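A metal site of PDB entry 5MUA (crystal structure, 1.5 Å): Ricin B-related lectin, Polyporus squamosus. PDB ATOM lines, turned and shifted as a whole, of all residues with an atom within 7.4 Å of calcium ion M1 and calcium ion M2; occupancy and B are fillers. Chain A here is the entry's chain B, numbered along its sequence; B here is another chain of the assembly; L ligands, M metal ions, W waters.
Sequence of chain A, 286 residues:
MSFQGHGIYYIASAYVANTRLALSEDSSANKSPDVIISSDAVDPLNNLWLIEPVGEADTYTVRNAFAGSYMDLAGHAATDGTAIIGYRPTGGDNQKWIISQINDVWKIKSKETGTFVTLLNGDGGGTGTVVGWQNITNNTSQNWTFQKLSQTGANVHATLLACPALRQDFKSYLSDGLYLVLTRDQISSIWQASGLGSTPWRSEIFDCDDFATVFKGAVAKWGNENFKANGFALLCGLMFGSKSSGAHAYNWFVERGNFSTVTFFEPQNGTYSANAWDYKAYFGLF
Calcium ion M1 is bound by the side-chain carboxylate (OD1) of Asp 207 (2.3 Å), the backbone carbonyl oxygen (O) of Glu 204 (2.4 Å), the side-chain carboxylate (OD2) of Asp 210 (2.4 Å), the side-chain carboxylate (OD1) of Asp 209 (2.4 Å), water W2 (2.5 Å), the side-chain carboxylate (OD2) of Asp 176 of chain B (2.5 Å), the side-chain carboxylate (OD2) of Asp 209 (2.6 Å) and the side-chain carboxylate (OD1) of Asp 176 of chain B (2.6 Å).
Water W1 lies within hydrogen-bond range of a nitrogen (N2) of the ligand (3.2 Å) and the side-chain carboxylate (OE2) of Glu 204 (3.4 Å).
OD2 of Asp 176 of chain B sits close to OG of Ser 175 of chain B (2.8 Å). N of Asp 176 of chain B is in hydrogen-bond range of OH of Tyr 179 of chain B. The backbone carbonyl oxygen (O) of Arg 202 lies within hydrogen-bond range of the backbone NH (N) of Asp 207. OE1 of Glu 204 is in hydrogen-bond range of OG of Ser 203. The backbone NH of Ser 175 of chain B is in hydrogen-bond range of the side-chain hydroxyl of Tyr 179 of chain B (3.5 Å). The backbone NH (N) of Ser 175 of chain B is in hydrogen-bond range of the chain-end carboxylate (O) of Phe 286 of chain B (2.9 Å).
Calcium ion M2 is bound by an oxygen (O4) of the ligand (2.3 Å), the side-chain carboxylate of Asp 209 (2.3 Å), the side-chain carboxylate of Asp 176 of chain B (2.3 Å), the side-chain carboxylate of Asp 207 (2.5 Å), water W1 (2.5 Å) and the backbone carbonyl oxygen of Ser 175 of chain B (2.6 Å). Calcium ion M2 has six donor atoms within binding distance. Slightly farther from calcium ion M2 lies the side-chain carboxylate (OD1) of Asp 207 (3.0 Å).
Within 4 Å of calcium ion M1: Glu 204, Asp 207, Asp 209, Asp 210 and Asp 176 of chain B. The nearest printed residue that does not touch calcium ion M1 is Ala 233 of chain B (4.3 Å).
The backbone NH of Cys 208 sits at hydrogen-bond distance from an oxygen (O1) of the ligand (2.9 Å). The side-chain sulfur of Cys 208 is covalently linked to a carbon (C2) of the ligand, 1.9 Å away. An oxygen (O1) of the ligand is in hydrogen-bond range of the indole nitrogen (NE1) of Trp 201, at 2.7 Å.
The nearest printed residue that does not touch calcium ion M2 is Glu 204 (4.4 Å).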
ATOM      1  N   TRP A 201      24.764 -16.273 -17.386  1.00  0.00           N
ATOM      2  CA  TRP A 201      23.976 -16.120 -18.543  1.00  0.00           C
ATOM      3  C   TRP A 201      23.983 -17.443 -19.274  1.00  0.00           C
ATOM      4  O   TRP A 201      25.039 -17.996 -19.540  1.00  0.00           O
ATOM      5  CB  TRP A 201      24.470 -15.017 -19.443  1.00  0.00           C
ATOM      6  CG  TRP A 201      23.758 -14.749 -20.690  1.00  0.00           C
ATOM      7  CD1 TRP A 201      22.821 -13.745 -20.905  1.00  0.00           C
ATOM      8  CD2 TRP A 201      23.886 -15.405 -21.971  1.00  0.00           C
ATOM      9  NE1 TRP A 201      22.358 -13.754 -22.165  1.00  0.00           N
ATOM     10  CE2 TRP A 201      22.955 -14.775 -22.860  1.00  0.00           C
ATOM     11  CE3 TRP A 201      24.647 -16.458 -22.462  1.00  0.00           C
ATOM     12  CZ2 TRP A 201      22.785 -15.164 -24.176  1.00  0.00           C
ATOM     13  CZ3 TRP A 201      24.467 -16.869 -23.778  1.00  0.00           C
ATOM     14  CH2 TRP A 201      23.555 -16.190 -24.631  1.00  0.00           C
ATOM     15  N   ARG A 202      22.794 -17.909 -19.659  1.00  0.00           N
ATOM     16  CA  ARG A 202      22.745 -19.116 -20.531  1.00  0.00           C
ATOM     17  C   ARG A 202      21.696 -18.892 -21.556  1.00  0.00           C
ATOM     18  O   ARG A 202      20.524 -18.464 -21.249  1.00  0.00           O
ATOM     19  CB  ARG A 202      22.526 -20.383 -19.734  1.00  0.00           C
ATOM     20  CG  ARG A 202      23.515 -20.587 -18.574  1.00  0.00           C
ATOM     21  CD  ARG A 202      23.439 -21.996 -17.954  1.00  0.00           C
ATOM     22  NE  ARG A 202      22.261 -22.106 -17.057  1.00  0.00           N
ATOM     23  CZ  ARG A 202      21.342 -23.058 -17.113  1.00  0.00           C
ATOM     24  NH1 ARG A 202      21.467 -24.071 -18.004  1.00  0.00           N
ATOM     25  NH2 ARG A 202      20.330 -23.054 -16.275  1.00  0.00           N
ATOM     26  N   SER A 203      22.045 -19.241 -22.788  1.00  0.00           N
ATOM     27  CA  SER A 203      21.224 -18.972 -23.931  1.00  0.00           C
ATOM     28  C   SER A 203      19.846 -19.615 -23.805  1.00  0.00           C
ATOM     29  O   SER A 203      19.769 -20.779 -23.465  1.00  0.00           O
ATOM     30  CB  SER A 203      21.916 -19.426 -25.203  1.00  0.00           C
ATOM     31  OG  SER A 203      21.199 -18.967 -26.319  1.00  0.00           O
ATOM     32  N   GLU A 204      18.806 -18.833 -24.074  1.00  0.00           N
ATOM     33  CA  GLU A 204      17.350 -19.232 -23.945  1.00  0.00           C
ATOM     34  C   GLU A 204      16.854 -19.524 -22.542  1.00  0.00           C
ATOM     35  O   GLU A 204      15.829 -18.963 -22.093  1.00  0.00           O
ATOM     36  CB  GLU A 204      16.988 -20.359 -24.903  1.00  0.00           C
ATOM     37  CG  GLU A 204      16.939 -19.959 -26.393  1.00  0.00           C
ATOM     38  CD  GLU A 204      18.307 -19.773 -27.032  1.00  0.00           C
ATOM     39  OE1 GLU A 204      19.247 -20.537 -26.695  1.00  0.00           O
ATOM     40  OE2 GLU A 204      18.407 -18.859 -27.894  1.00  0.00           O
ATOM     41  N   ILE A 205      17.551 -20.393 -21.814  1.00  0.00           N
ATOM     42  CA  ILE A 205      17.071 -20.907 -20.570  1.00  0.00           C
ATOM     43  C   ILE A 205      17.209 -19.879 -19.409  1.00  0.00           C
ATOM     44  O   ILE A 205      16.407 -19.864 -18.515  1.00  0.00           O
ATOM     45  CB  ILE A 205      17.799 -22.241 -20.293  1.00  0.00           C
ATOM     46  CG1 ILE A 205      17.117 -23.034 -19.197  1.00  0.00           C
ATOM     47  CG2 ILE A 205      19.307 -22.050 -19.990  1.00  0.00           C
ATOM     48  CD1 ILE A 205      15.646 -23.395 -19.408  1.00  0.00           C
ATOM     49  N   PHE A 206      18.221 -19.048 -19.507  1.00  0.00           N
ATOM     50  CA  PHE A 206      18.342 -17.906 -18.614  1.00  0.00           C
ATOM     51  C   PHE A 206      19.199 -16.806 -19.245  1.00  0.00           C
ATOM     52  O   PHE A 206      20.326 -16.588 -18.906  1.00  0.00           O
ATOM     53  CB  PHE A 206      18.829 -18.295 -17.231  1.00  0.00           C
ATOM     54  CG  PHE A 206      18.299 -17.373 -16.185  1.00  0.00           C
ATOM     55  CD1 PHE A 206      17.011 -17.577 -15.658  1.00  0.00           C
ATOM     56  CD2 PHE A 206      19.028 -16.304 -15.773  1.00  0.00           C
ATOM     57  CE1 PHE A 206      16.452 -16.744 -14.702  1.00  0.00           C
ATOM     58  CE2 PHE A 206      18.458 -15.419 -14.834  1.00  0.00           C
ATOM     59  CZ  PHE A 206      17.200 -15.644 -14.308  1.00  0.00           C
ATOM     60  N   ASP A 207      18.555 -16.104 -20.171  1.00  0.00           N
ATOM     61  CA  ASP A 207      19.133 -15.098 -21.010  1.00  0.00           C
ATOM     62  C   ASP A 207      18.448 -13.700 -20.773  1.00  0.00           C
ATOM     63  O   ASP A 207      17.783 -13.529 -19.735  1.00  0.00           O
ATOM     64  CB  ASP A 207      19.334 -15.553 -22.438  1.00  0.00           C
ATOM     65  CG  ASP A 207      18.038 -15.927 -23.143  1.00  0.00           C
ATOM     66  OD1 ASP A 207      16.966 -15.964 -22.448  1.00  0.00           O
ATOM     67  OD2 ASP A 207      18.089 -16.035 -24.401  1.00  0.00           O
ATOM     68  N   CYS A 208      18.686 -12.709 -21.644  1.00  0.00           N
ATOM     69  CA  CYS A 208      18.354 -11.345 -21.253  1.00  0.00           C
ATOM     70  C   CYS A 208      16.864 -11.246 -20.892  1.00  0.00           C
ATOM     71  O   CYS A 208      16.521 -10.559 -19.904  1.00  0.00           O
ATOM     72  CB  CYS A 208      18.630 -10.374 -22.349  1.00  0.00           C
ATOM     73  SG  CYS A 208      17.862 -10.627 -23.962  1.00  0.00           S
ATOM     74  N   ASP A 209      15.998 -11.922 -21.618  1.00  0.00           N
ATOM     75  CA  ASP A 209      14.619 -11.868 -21.272  1.00  0.00           C
ATOM     76  C   ASP A 209      14.359 -12.305 -19.837  1.00  0.00           C
ATOM     77  O   ASP A 209      13.496 -11.722 -19.156  1.00  0.00           O
ATOM     78  CB  ASP A 209      13.702 -12.575 -22.269  1.00  0.00           C
ATOM     79  CG  ASP A 209      13.982 -14.091 -22.410  1.00  0.00           C
ATOM     80  OD1 ASP A 209      13.426 -14.881 -21.619  1.00  0.00           O
ATOM     81  OD2 ASP A 209      14.824 -14.426 -23.289  1.00  0.00           O
ATOM     82  N   ASP A 210      15.067 -13.301 -19.365  1.00  0.00           N
ATOM     83  CA  ASP A 210      14.839 -13.848 -18.043  1.00  0.00           C
ATOM     84  C   ASP A 210      15.389 -12.890 -16.963  1.00  0.00           C
ATOM     85  O   ASP A 210      14.740 -12.629 -15.992  1.00  0.00           O
ATOM     86  CB  ASP A 210      15.457 -15.225 -17.931  1.00  0.00           C
ATOM     87  CG  ASP A 210      14.848 -16.163 -18.920  1.00  0.00           C
ATOM     88  OD1 ASP A 210      13.650 -16.482 -18.736  1.00  0.00           O
ATOM     89  OD2 ASP A 210      15.517 -16.445 -19.936  1.00  0.00           O
ATOM     90  N   PHE A 211      16.589 -12.356 -17.195  1.00  0.00           N
ATOM     91  CA  PHE A 211      17.146 -11.369 -16.281  1.00  0.00           C
ATOM     92  C   PHE A 211      16.188 -10.203 -16.131  1.00  0.00           C
ATOM     93  O   PHE A 211      15.946  -9.810 -14.981  1.00  0.00           O
ATOM     94  CB  PHE A 211      18.495 -10.855 -16.752  1.00  0.00           C
ATOM     95  CG  PHE A 211      19.630 -11.826 -16.503  1.00  0.00           C
ATOM     96  CD1 PHE A 211      20.304 -11.831 -15.289  1.00  0.00           C
ATOM     97  CD2 PHE A 211      19.972 -12.773 -17.467  1.00  0.00           C
ATOM     98  CE1 PHE A 211      21.297 -12.740 -15.039  1.00  0.00           C
ATOM     99  CE2 PHE A 211      20.986 -13.680 -17.239  1.00  0.00           C
ATOM    100  CZ  PHE A 211      21.639 -13.678 -15.998  1.00  0.00           C
ATOM    101  N   LEU B 174       7.696 -12.305 -28.321  1.00  0.00           N
ATOM    102  CA  LEU B 174       8.262 -13.494 -27.787  1.00  0.00           C
ATOM    103  C   LEU B 174       9.770 -13.360 -27.636  1.00  0.00           C
ATOM    104  O   LEU B 174      10.387 -12.555 -28.276  1.00  0.00           O
ATOM    105  CB  LEU B 174       7.945 -14.751 -28.621  1.00  0.00           C
ATOM    106  CG  LEU B 174       8.371 -14.764 -30.111  1.00  0.00           C
ATOM    107  CD1 LEU B 174       8.764 -16.180 -30.484  1.00  0.00           C
ATOM    108  CD2 LEU B 174       7.178 -14.411 -31.043  1.00  0.00           C
ATOM    109  N   SER B 175      10.317 -14.195 -26.763  1.00  0.00           N
ATOM    110  CA  SER B 175      11.687 -14.036 -26.339  1.00  0.00           C
ATOM    111  C   SER B 175      12.610 -15.125 -26.751  1.00  0.00           C
ATOM    112  O   SER B 175      13.823 -14.883 -26.717  1.00  0.00           O
ATOM    113  CB  SER B 175      11.745 -13.809 -24.843  1.00  0.00           C
ATOM    114  OG  SER B 175      11.300 -14.923 -24.096  1.00  0.00           O
ATOM    115  N   ASP B 176      12.097 -16.338 -27.086  1.00  0.00           N
ATOM    116  CA  ASP B 176      12.985 -17.493 -27.261  1.00  0.00           C
ATOM    117  C   ASP B 176      12.510 -18.318 -28.444  1.00  0.00           C
ATOM    118  O   ASP B 176      11.372 -18.236 -28.842  1.00  0.00           O
ATOM    119  CB  ASP B 176      13.016 -18.335 -26.007  1.00  0.00           C
ATOM    120  CG  ASP B 176      13.624 -17.577 -24.796  1.00  0.00           C
ATOM    121  OD1 ASP B 176      14.869 -17.406 -24.776  1.00  0.00           O
ATOM    122  OD2 ASP B 176      12.900 -17.193 -23.850  1.00  0.00           O
ATOM    123  N   GLY B 177      13.439 -19.060 -29.050  1.00  0.00           N
ATOM    124  CA  GLY B 177      13.128 -19.727 -30.313  1.00  0.00           C
ATOM    125  C   GLY B 177      12.657 -21.149 -30.172  1.00  0.00           C
ATOM    126  O   GLY B 177      12.186 -21.738 -31.178  1.00  0.00           O
ATOM    127  N   TYR B 179      10.714 -23.728 -27.077  1.00  0.00           N
ATOM    128  CA  TYR B 179      10.112 -23.866 -25.784  1.00  0.00           C
ATOM    129  C   TYR B 179       9.795 -25.326 -25.408  1.00  0.00           C
ATOM    130  O   TYR B 179       9.261 -26.061 -26.240  1.00  0.00           O
ATOM    131  CB  TYR B 179       8.757 -23.160 -25.813  1.00  0.00           C
ATOM    132  CG  TYR B 179       8.936 -21.650 -25.879  1.00  0.00           C
ATOM    133  CD1 TYR B 179       9.233 -20.915 -24.749  1.00  0.00           C
ATOM    134  CD2 TYR B 179       8.831 -20.976 -27.071  1.00  0.00           C
ATOM    135  CE1 TYR B 179       9.416 -19.535 -24.825  1.00  0.00           C
ATOM    136  CE2 TYR B 179       9.044 -19.613 -27.156  1.00  0.00           C
ATOM    137  CZ  TYR B 179       9.312 -18.888 -26.008  1.00  0.00           C
ATOM    138  OH  TYR B 179       9.435 -17.523 -26.146  1.00  0.00           O
ATOM    139  N   ALA B 220      10.696 -19.123 -14.960  1.00  0.00           N
ATOM    140  CA  ALA B 220      12.037 -18.980 -15.474  1.00  0.00           C
ATOM    141  C   ALA B 220      13.101 -19.391 -14.477  1.00  0.00           C
ATOM    142  O   ALA B 220      14.091 -20.071 -14.851  1.00  0.00           O
ATOM    143  CB  ALA B 220      12.254 -17.537 -15.912  1.00  0.00           C
ATOM    144  N   PHE B 232      16.911 -23.775 -25.015  1.00  0.00           N
ATOM    145  CA  PHE B 232      15.472 -23.806 -24.968  1.00  0.00           C
ATOM    146  C   PHE B 232      15.017 -22.995 -23.723  1.00  0.00           C
ATOM    147  O   PHE B 232      15.811 -22.792 -22.777  1.00  0.00           O
ATOM    148  CB  PHE B 232      14.941 -25.248 -24.836  1.00  0.00           C
ATOM    149  CG  PHE B 232      15.166 -25.856 -23.479  1.00  0.00           C
ATOM    150  CD1 PHE B 232      16.395 -26.287 -23.115  1.00  0.00           C
ATOM    151  CD2 PHE B 232      14.120 -26.023 -22.615  1.00  0.00           C
ATOM    152  CE1 PHE B 232      16.596 -26.837 -21.874  1.00  0.00           C
ATOM    153  CE2 PHE B 232      14.282 -26.610 -21.414  1.00  0.00           C
ATOM    154  CZ  PHE B 232      15.550 -26.987 -21.001  1.00  0.00           C
ATOM    155  N   ALA B 233      13.752 -22.580 -23.746  1.00  0.00           N
ATOM    156  CA  ALA B 233      13.101 -21.895 -22.638  1.00  0.00           C
ATOM    157  C   ALA B 233      11.871 -22.683 -22.219  1.00  0.00           C
ATOM    158  O   ALA B 233      11.340 -23.518 -22.967  1.00  0.00           O
ATOM    159  CB  ALA B 233      12.698 -20.491 -23.101  1.00  0.00           C
ATOM    160  N   LEU B 234      11.351 -22.339 -21.030  1.00  0.00           N
ATOM    161  CA  LEU B 234      10.053 -22.861 -20.565  1.00  0.00           C
ATOM    162  C   LEU B 234       8.948 -21.986 -20.997  1.00  0.00           C
ATOM    163  O   LEU B 234       9.000 -20.778 -20.765  1.00  0.00           O
ATOM    164  CB  LEU B 234      10.055 -23.044 -19.041  1.00  0.00           C
ATOM    165  CG  LEU B 234      11.218 -23.820 -18.447  1.00  0.00           C
ATOM    166  CD1 LEU B 234      10.843 -24.126 -17.010  1.00  0.00           C
ATOM    167  CD2 LEU B 234      11.492 -25.084 -19.211  1.00  0.00           C
ATOM    168  N   PHE B 286       5.676 -14.027 -24.181  1.00  0.00           N
ATOM    169  CA  PHE B 286       6.124 -15.371 -23.879  1.00  0.00           C
ATOM    170  C   PHE B 286       7.559 -15.628 -24.330  1.00  0.00           C
ATOM    171  O   PHE B 286       8.110 -14.647 -24.923  1.00  0.00           O
ATOM    172  CB  PHE B 286       5.193 -16.430 -24.495  1.00  0.00           C
ATOM    173  CG  PHE B 286       5.241 -16.542 -25.968  1.00  0.00           C
ATOM    174  CD1 PHE B 286       4.484 -15.679 -26.753  1.00  0.00           C
ATOM    175  CD2 PHE B 286       5.950 -17.569 -26.579  1.00  0.00           C
ATOM    176  CE1 PHE B 286       4.444 -15.803 -28.096  1.00  0.00           C
ATOM    177  CE2 PHE B 286       5.930 -17.688 -27.930  1.00  0.00           C
ATOM    178  CZ  PHE B 286       5.153 -16.826 -28.693  1.00  0.00           C
ATOM    179  OXT PHE B 286       8.050 -16.759 -24.112  1.00  0.00           O
HETATM  180  C1  LIG L   1      20.485 -11.426 -24.475  1.00  0.00           C
HETATM  181  O1  LIG L   1      20.705 -12.382 -23.733  1.00  0.00           O
HETATM  182  O2  LIG L   1      21.291 -10.462 -24.646  1.00  0.00           O
HETATM  183  C2  LIG L   1      19.154 -11.322 -25.104  1.00  0.00           C
HETATM  184  C3  LIG L   1      18.743 -12.673 -25.669  1.00  0.00           C
HETATM  185  O3  LIG L   1      19.664 -12.723 -26.753  1.00  0.00           O
HETATM  186  C4  LIG L   1      17.348 -12.698 -26.182  1.00  0.00           C
HETATM  187  O4  LIG L   1      16.459 -13.162 -25.542  1.00  0.00           O
HETATM  188  N1  LIG L   1      17.106 -12.097 -27.307  1.00  0.00           N
HETATM  189  C5  LIG L   1      15.805 -12.010 -27.945  1.00  0.00           C
HETATM  190  C6  LIG L   1      15.031 -10.707 -27.922  1.00  0.00           C
HETATM  191  C7  LIG L   1      14.894 -10.079 -26.542  1.00  0.00           C
HETATM  192  C8  LIG L   1      13.879 -10.867 -25.715  1.00  0.00           C
HETATM  193  C9  LIG L   1      14.456  -8.691 -26.732  1.00  0.00           C
HETATM  194  C10 LIG L   1      15.657 -12.773 -29.251  1.00  0.00           C
HETATM  195  O5  LIG L   1      16.028 -12.193 -30.257  1.00  0.00           O
HETATM  196  N2  LIG L   1      15.167 -13.989 -29.296  1.00  0.00           N
HETATM  197  C11 LIG L   1      14.808 -14.697 -30.546  1.00  0.00           C
HETATM  198  C12 LIG L   1      13.317 -14.993 -30.554  1.00  0.00           C
HETATM  199  C13 LIG L   1      12.824 -15.881 -31.724  1.00  0.00           C
HETATM  200  C14 LIG L   1      11.740 -15.146 -32.520  1.00  0.00           C
HETATM  201  N3  LIG L   1      11.024 -16.129 -33.339  1.00  0.00           N
HETATM  202  C15 LIG L   1       9.929 -15.900 -34.045  1.00  0.00           C
HETATM  203  N4  LIG L   1       9.464 -14.639 -34.209  1.00  0.00           N
HETATM  204  N5  LIG L   1       9.249 -16.975 -34.575  1.00  0.00           N
HETATM  205 CA    CA M   1      14.785 -16.804 -22.221  1.00  0.00          CA
HETATM  206 CA    CA M   2      15.845 -15.321 -25.177  1.00  0.00          CA
HETATM  207  O   HOH W   1      16.940 -15.847 -27.407  1.00  0.00           O
HETATM  208  O   HOH W   2      13.005 -17.891 -20.851  1.00  0.00           O
